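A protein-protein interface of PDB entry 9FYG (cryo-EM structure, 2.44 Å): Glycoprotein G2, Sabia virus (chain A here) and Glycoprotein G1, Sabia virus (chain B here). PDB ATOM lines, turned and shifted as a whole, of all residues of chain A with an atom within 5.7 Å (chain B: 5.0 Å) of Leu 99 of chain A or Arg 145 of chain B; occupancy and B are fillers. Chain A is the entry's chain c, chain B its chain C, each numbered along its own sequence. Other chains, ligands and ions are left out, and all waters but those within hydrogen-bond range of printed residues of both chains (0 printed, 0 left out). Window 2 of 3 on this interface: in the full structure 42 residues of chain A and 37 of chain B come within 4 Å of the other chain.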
ATOM      1  N   ASN A  94      11.650  32.918   0.139  1.00  0.00           N
ATOM      2  CA  ASN A  94      10.358  32.509   0.682  1.00  0.00           C
ATOM      3  C   ASN A  94      10.334  31.018   0.999  1.00  0.00           C
ATOM      4  O   ASN A  94       9.782  30.605   2.026  1.00  0.00           O
ATOM      5  CB  ASN A  94       9.239  32.883  -0.288  1.00  0.00           C
ATOM      6  CG  ASN A  94       8.802  34.326  -0.137  1.00  0.00           C
ATOM      7  OD1 ASN A  94       8.522  34.786   0.966  1.00  0.00           O
ATOM      8  ND2 ASN A  94       8.754  35.048  -1.245  1.00  0.00           N
ATOM      9  N   ARG A  95      10.941  30.195   0.141  1.00  0.00           N
ATOM     10  CA  ARG A  95      11.001  28.763   0.416  1.00  0.00           C
ATOM     11  C   ARG A  95      11.826  28.476   1.665  1.00  0.00           C
ATOM     12  O   ARG A  95      11.460  27.618   2.476  1.00  0.00           O
ATOM     13  CB  ARG A  95      11.571  28.019  -0.793  1.00  0.00           C
ATOM     14  CG  ARG A  95      11.690  26.521  -0.590  1.00  0.00           C
ATOM     15  CD  ARG A  95      10.324  25.859  -0.552  1.00  0.00           C
ATOM     16  NE  ARG A  95       9.943  25.310  -1.848  1.00  0.00           N
ATOM     17  CZ  ARG A  95       8.716  24.921  -2.165  1.00  0.00           C
ATOM     18  NH1 ARG A  95       7.715  25.027  -1.309  1.00  0.00           N
ATOM     19  NH2 ARG A  95       8.489  24.414  -3.373  1.00  0.00           N
ATOM     20  N   LEU A  96      12.944  29.184   1.837  1.00  0.00           N
ATOM     21  CA  LEU A  96      13.779  28.980   3.016  1.00  0.00           C
ATOM     22  C   LEU A  96      13.064  29.424   4.283  1.00  0.00           C
ATOM     23  O   LEU A  96      13.212  28.795   5.336  1.00  0.00           O
ATOM     24  CB  LEU A  96      15.108  29.716   2.852  1.00  0.00           C
ATOM     25  CG  LEU A  96      16.084  29.116   1.836  1.00  0.00           C
ATOM     26  CD1 LEU A  96      17.365  29.932   1.765  1.00  0.00           C
ATOM     27  CD2 LEU A  96      16.386  27.664   2.162  1.00  0.00           C
ATOM     28  N   LYS A  97      12.289  30.510   4.207  1.00  0.00           N
ATOM     29  CA  LYS A  97      11.463  30.898   5.345  1.00  0.00           C
ATOM     30  C   LYS A  97      10.422  29.829   5.653  1.00  0.00           C
ATOM     31  O   LYS A  97      10.138  29.546   6.823  1.00  0.00           O
ATOM     32  CB  LYS A  97      10.786  32.241   5.075  1.00  0.00           C
ATOM     33  CG  LYS A  97      11.736  33.418   5.035  1.00  0.00           C
ATOM     34  CD  LYS A  97      10.985  34.711   4.789  1.00  0.00           C
ATOM     35  CE  LYS A  97      11.933  35.893   4.726  1.00  0.00           C
ATOM     36  NZ  LYS A  97      11.207  37.170   4.492  1.00  0.00           N
ATOM     37  N   GLU A  98       9.834  29.233   4.614  1.00  0.00           N
ATOM     38  CA  GLU A  98       8.862  28.164   4.825  1.00  0.00           C
ATOM     39  C   GLU A  98       9.499  26.955   5.501  1.00  0.00           C
ATOM     40  O   GLU A  98       8.888  26.328   6.373  1.00  0.00           O
ATOM     41  CB  GLU A  98       8.233  27.765   3.491  1.00  0.00           C
ATOM     42  CG  GLU A  98       7.394  26.504   3.546  1.00  0.00           C
ATOM     43  CD  GLU A  98       6.820  26.138   2.198  1.00  0.00           C
ATOM     44  OE1 GLU A  98       7.225  26.759   1.195  1.00  0.00           O
ATOM     45  OE2 GLU A  98       5.961  25.234   2.140  1.00  0.00           O
ATOM     46  N   LEU A  99      10.728  26.610   5.109  1.00  0.00           N
ATOM     47  CA  LEU A  99      11.381  25.435   5.678  1.00  0.00           C
ATOM     48  C   LEU A  99      11.752  25.642   7.141  1.00  0.00           C
ATOM     49  O   LEU A  99      11.872  24.667   7.891  1.00  0.00           O
ATOM     50  CB  LEU A  99      12.624  25.075   4.863  1.00  0.00           C
ATOM     51  CG  LEU A  99      12.367  24.681   3.407  1.00  0.00           C
ATOM     52  CD1 LEU A  99      13.668  24.422   2.667  1.00  0.00           C
ATOM     53  CD2 LEU A  99      11.443  23.480   3.326  1.00  0.00           C
ATOM     54  N   LEU A 100      11.932  26.891   7.567  1.00  0.00           N
ATOM     55  CA  LEU A 100      12.334  27.211   8.928  1.00  0.00           C
ATOM     56  C   LEU A 100      11.154  27.543   9.835  1.00  0.00           C
ATOM     57  O   LEU A 100      11.366  27.989  10.967  1.00  0.00           O
ATOM     58  CB  LEU A 100      13.330  28.371   8.922  1.00  0.00           C
ATOM     59  CG  LEU A 100      14.654  28.113   8.204  1.00  0.00           C
ATOM     60  CD1 LEU A 100      15.421  29.410   8.022  1.00  0.00           C
ATOM     61  CD2 LEU A 100      15.484  27.095   8.964  1.00  0.00           C
ATOM     62  N   ASN A 101       9.923  27.349   9.358  1.00  0.00           N
ATOM     63  CA  ASN A 101       8.708  27.570  10.147  1.00  0.00           C
ATOM     64  C   ASN A 101       8.553  29.027  10.578  1.00  0.00           C
ATOM     65  O   ASN A 101       8.040  29.315  11.661  1.00  0.00           O
ATOM     66  CB  ASN A 101       8.660  26.643  11.366  1.00  0.00           C
ATOM     67  CG  ASN A 101       8.315  25.216  10.997  1.00  0.00           C
ATOM     68  OD1 ASN A 101       9.068  24.288  11.290  1.00  0.00           O
ATOM     69  ND2 ASN A 101       7.171  25.032  10.351  1.00  0.00           N
ATOM     70  N   TYR A 104       6.122  33.381   5.644  1.00  0.00           N
ATOM     71  CA  TYR A 104       6.646  33.376   4.287  1.00  0.00           C
ATOM     72  C   TYR A 104       5.514  33.639   3.308  1.00  0.00           C
ATOM     73  O   TYR A 104       4.333  33.491   3.631  1.00  0.00           O
ATOM     74  CB  TYR A 104       7.338  32.045   3.953  1.00  0.00           C
ATOM     75  CG  TYR A 104       6.391  30.874   3.824  1.00  0.00           C
ATOM     76  CD1 TYR A 104       5.908  30.221   4.948  1.00  0.00           C
ATOM     77  CD2 TYR A 104       5.976  30.426   2.577  1.00  0.00           C
ATOM     78  CE1 TYR A 104       5.040  29.157   4.835  1.00  0.00           C
ATOM     79  CE2 TYR A 104       5.108  29.365   2.457  1.00  0.00           C
ATOM     80  CZ  TYR A 104       4.645  28.732   3.589  1.00  0.00           C
ATOM     81  OH  TYR A 104       3.781  27.670   3.476  1.00  0.00           O
ATOM     82  N   ASN A 132       0.682  26.350   7.583  1.00  0.00           N
ATOM     83  CA  ASN A 132      -0.341  26.182   6.549  1.00  0.00           C
ATOM     84  C   ASN A 132      -1.592  26.998   6.867  1.00  0.00           C
ATOM     85  O   ASN A 132      -2.717  26.579   6.592  1.00  0.00           O
ATOM     86  CB  ASN A 132      -0.689  24.705   6.347  1.00  0.00           C
ATOM     87  CG  ASN A 132       0.532  23.850   6.064  1.00  0.00           C
ATOM     88  OD1 ASN A 132       0.995  23.105   6.926  1.00  0.00           O
ATOM     89  ND2 ASN A 132       1.062  23.959   4.852  1.00  0.00           N
ATOM     90  N   HIS B  31       6.481  14.174   3.992  1.00  0.00           N
ATOM     91  CA  HIS B  31       7.845  14.675   3.876  1.00  0.00           C
ATOM     92  C   HIS B  31       8.778  13.712   3.156  1.00  0.00           C
ATOM     93  O   HIS B  31       9.912  14.091   2.848  1.00  0.00           O
ATOM     94  CB  HIS B  31       8.396  15.010   5.264  1.00  0.00           C
ATOM     95  CG  HIS B  31       7.981  16.358   5.762  1.00  0.00           C
ATOM     96  ND1 HIS B  31       7.875  17.457   4.936  1.00  0.00           N
ATOM     97  CD2 HIS B  31       7.631  16.785   6.999  1.00  0.00           C
ATOM     98  CE1 HIS B  31       7.485  18.502   5.643  1.00  0.00           C
ATOM     99  NE2 HIS B  31       7.330  18.121   6.898  1.00  0.00           N
ATOM    100  N   TYR B  34       6.625  12.272  -2.865  1.00  0.00           N
ATOM    101  CA  TYR B  34       6.443  13.414  -3.750  1.00  0.00           C
ATOM    102  C   TYR B  34       5.966  12.912  -5.099  1.00  0.00           C
ATOM    103  O   TYR B  34       6.267  11.787  -5.490  1.00  0.00           O
ATOM    104  CB  TYR B  34       7.773  14.165  -3.882  1.00  0.00           C
ATOM    105  CG  TYR B  34       8.108  14.833  -2.594  1.00  0.00           C
ATOM    106  CD1 TYR B  34       7.095  15.265  -1.764  1.00  0.00           C
ATOM    107  CD2 TYR B  34       9.408  14.859  -2.105  1.00  0.00           C
ATOM    108  CE1 TYR B  34       7.361  15.819  -0.563  1.00  0.00           C
ATOM    109  CE2 TYR B  34       9.671  15.424  -0.874  1.00  0.00           C
ATOM    110  CZ  TYR B  34       8.631  15.900  -0.115  1.00  0.00           C
ATOM    111  OH  TYR B  34       8.818  16.463   1.123  1.00  0.00           O
ATOM    112  N   GLY B 139      13.790  19.734  -0.087  1.00  0.00           N
ATOM    113  CA  GLY B 139      13.089  20.780   0.641  1.00  0.00           C
ATOM    114  C   GLY B 139      12.818  22.009  -0.207  1.00  0.00           C
ATOM    115  O   GLY B 139      11.744  22.607  -0.128  1.00  0.00           O
ATOM    116  N   VAL B 140      13.794  22.409  -1.018  1.00  0.00           N
ATOM    117  CA  VAL B 140      13.612  23.565  -1.890  1.00  0.00           C
ATOM    118  C   VAL B 140      12.563  23.277  -2.960  1.00  0.00           C
ATOM    119  O   VAL B 140      11.715  24.124  -3.263  1.00  0.00           O
ATOM    120  CB  VAL B 140      14.961  23.977  -2.509  1.00  0.00           C
ATOM    121  CG1 VAL B 140      14.755  24.910  -3.690  1.00  0.00           C
ATOM    122  CG2 VAL B 140      15.844  24.624  -1.459  1.00  0.00           C
ATOM    123  N   GLY B 143       9.120  21.670  -0.687  1.00  0.00           N
ATOM    124  CA  GLY B 143       8.759  22.088   0.654  1.00  0.00           C
ATOM    125  C   GLY B 143       9.010  21.049   1.720  1.00  0.00           C
ATOM    126  O   GLY B 143       8.264  20.975   2.696  1.00  0.00           O
ATOM    127  N   SER B 144      10.047  20.238   1.561  1.00  0.00           N
ATOM    128  CA  SER B 144      10.303  19.138   2.474  1.00  0.00           C
ATOM    129  C   SER B 144      11.088  19.605   3.691  1.00  0.00           C
ATOM    130  O   SER B 144      12.054  20.364   3.574  1.00  0.00           O
ATOM    131  CB  SER B 144      11.080  18.035   1.764  1.00  0.00           C
ATOM    132  OG  SER B 144      11.094  16.845   2.541  1.00  0.00           O
ATOM    133  N   ARG B 145      10.675  19.133   4.866  1.00  0.00           N
ATOM    134  CA  ARG B 145      11.448  19.306   6.087  1.00  0.00           C
ATOM    135  C   ARG B 145      12.222  18.045   6.451  1.00  0.00           C
ATOM    136  O   ARG B 145      12.625  17.881   7.606  1.00  0.00           O
ATOM    137  CB  ARG B 145      10.535  19.732   7.236  1.00  0.00           C
ATOM    138  CG  ARG B 145      10.427  21.238   7.382  1.00  0.00           C
ATOM    139  CD  ARG B 145       9.197  21.643   8.163  1.00  0.00           C
ATOM    140  NE  ARG B 145       8.727  22.964   7.770  1.00  0.00           N
ATOM    141  CZ  ARG B 145       7.472  23.243   7.447  1.00  0.00           C
ATOM    142  NH1 ARG B 145       6.531  22.314   7.474  1.00  0.00           N
ATOM    143  NH2 ARG B 145       7.155  24.483   7.091  1.00  0.00           N
ATOM    144  N   ILE B 146      12.438  17.153   5.481  1.00  0.00           N
ATOM    145  CA  ILE B 146      13.147  15.907   5.749  1.00  0.00           C
ATOM    146  C   ILE B 146      14.611  16.170   6.090  1.00  0.00           C
ATOM    147  O   ILE B 146      15.201  15.450   6.904  1.00  0.00           O
ATOM    148  CB  ILE B 146      12.995  14.942   4.556  1.00  0.00           C
ATOM    149  CG1 ILE B 146      13.448  13.533   4.943  1.00  0.00           C
ATOM    150  CG2 ILE B 146      13.767  15.438   3.334  1.00  0.00           C
ATOM    151  CD1 ILE B 146      12.808  12.456   4.117  1.00  0.00           C
ATOM    152  N   ALA B 147      15.222  17.191   5.480  1.00  0.00           N
ATOM    153  CA  ALA B 147      16.607  17.522   5.793  1.00  0.00           C
ATOM    154  C   ALA B 147      16.752  18.027   7.220  1.00  0.00           C
ATOM    155  O   ALA B 147      17.829  17.907   7.812  1.00  0.00           O
ATOM    156  CB  ALA B 147      17.138  18.563   4.810  1.00  0.00           C
ATOM    157  N   PHE B 148      15.690  18.593   7.782  1.00  0.00           N
ATOM    158  CA  PHE B 148      15.699  19.123   9.144  1.00  0.00           C
ATOM    159  C   PHE B 148      15.218  18.079  10.147  1.00  0.00           C
ATOM    160  O   PHE B 148      14.306  18.312  10.937  1.00  0.00           O
ATOM    161  CB  PHE B 148      14.849  20.386   9.207  1.00  0.00           C
ATOM    162  CG  PHE B 148      15.168  21.385   8.130  1.00  0.00           C
ATOM    163  CD1 PHE B 148      14.566  21.302   6.884  1.00  0.00           C
ATOM    164  CD2 PHE B 148      16.077  22.403   8.360  1.00  0.00           C
ATOM    165  CE1 PHE B 148      14.863  22.213   5.892  1.00  0.00           C
ATOM    166  CE2 PHE B 148      16.376  23.321   7.371  1.00  0.00           C
ATOM    167  CZ  PHE B 148      15.768  23.225   6.136  1.00  0.00           C
ATOM    168  N   SER B 149      15.845  16.906  10.117  1.00  0.00           N
ATOM    169  CA  SER B 149      15.456  15.796  10.973  1.00  0.00           C
ATOM    170  C   SER B 149      16.691  14.969  11.298  1.00  0.00           C
ATOM    171  O   SER B 149      17.751  15.128  10.688  1.00  0.00           O
ATOM    172  CB  SER B 149      14.380  14.927  10.314  1.00  0.00           C
ATOM    173  OG  SER B 149      13.264  15.704   9.916  1.00  0.00           O
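NE of Arg 95 of chain A lies within hydrogen-bond range of O of Val 140 of chain B, at 2.6 Å.
The backbone carbonyl oxygen (O) of Glu 98 of chain A sits at hydrogen-bond distance from the guanidinium group (NH2) of Arg 145 of chain B.
The side-chain amide nitrogen (ND2) of Asn 101 of chain A lies close to the guanidinium group (NH2) of Arg 145 of chain B.
O of His 31 of chain B is in hydrogen-bond range of OG of Ser 144 of chain B, 3.0 Å away.
The backbone NH (N) of Ile 146 of chain B lies close to the side-chain hydroxyl (OG) of Ser 144 of chain B.
OH of Tyr 34 of chain B sits at hydrogen-bond distance from OG of Ser 144 of chain B (2.7 Å).
NH1 of Arg 95 of chain A lies within salt-bridge range of OE1 of Glu 98 of chain A (3.1 Å).
The backbone carbonyl oxygen of Arg 145 of chain B lies within hydrogen-bond range of the side-chain hydroxyl of Ser 149 of chain B (3.2 Å).
The backbone NH of Arg 145 of chain B sits at hydrogen-bond distance from a ring nitrogen (ND1) of His 31 of chain B (3.3 Å).
Gly 139 of chain B touches Arg 95 of chain A.
Gly 143 of chain B touches Arg 95 of chain A (N to CZ, 3.6 Å).
CD2 of Leu 99 of chain A touches O of Gly 139 of chain B, 3.6 Å away.
CD2 of Leu 99 of chain A touches C of Gly 143 of chain B, at 3.8 Å.
Ser 144 of chain B touches Leu 99 of chain A (O to CD2, 3.2 Å).
O of Leu 99 of chain A touches NE of Arg 145 of chain B, 3.6 Å away.
Phe 148 of chain B touches Leu 99 of chain A (CE1 to CB, 3.8 Å).
Leu 99 of chain A touches just these residues of chain B: Gly 139 (3.6 Å), Gly 143 (3.8 Å), Ser 144 (3.2 Å), Arg 145 (3.6 Å) and Phe 148 (3.8 Å).
Printed residues of chain B within 4 Å of Asn 101 of chain A: Arg 145.
Tyr 34 of chain B touches none of the printed residues of chain A.
Printed residues of chain A within 4 Å of Gly 143 of chain B: Arg 95 and Leu 99.
Of chain A, only Glu 98, Leu 99 and Asn 101 come within 4 Å of Arg 145 of chain B.
The nearest residue of chain B that does not touch Leu 99 of chain A is Val 140 of chain B (4.2 Å).
Of the 11 printed residues of chain B, 6 touch a printed residue of chain A.
Hydrophobic or aromatic side chains of chain B within 4 Å of the printed part of chain A: Phe 148.
Hydrophobic or aromatic side chains of chain A within 4 Å of the printed part of chain B: Leu 99.
Among the printed residues, no Asp or Glu carboxylate lies within 4 Å of a Lys or Arg side-chain nitrogen of the other chain.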
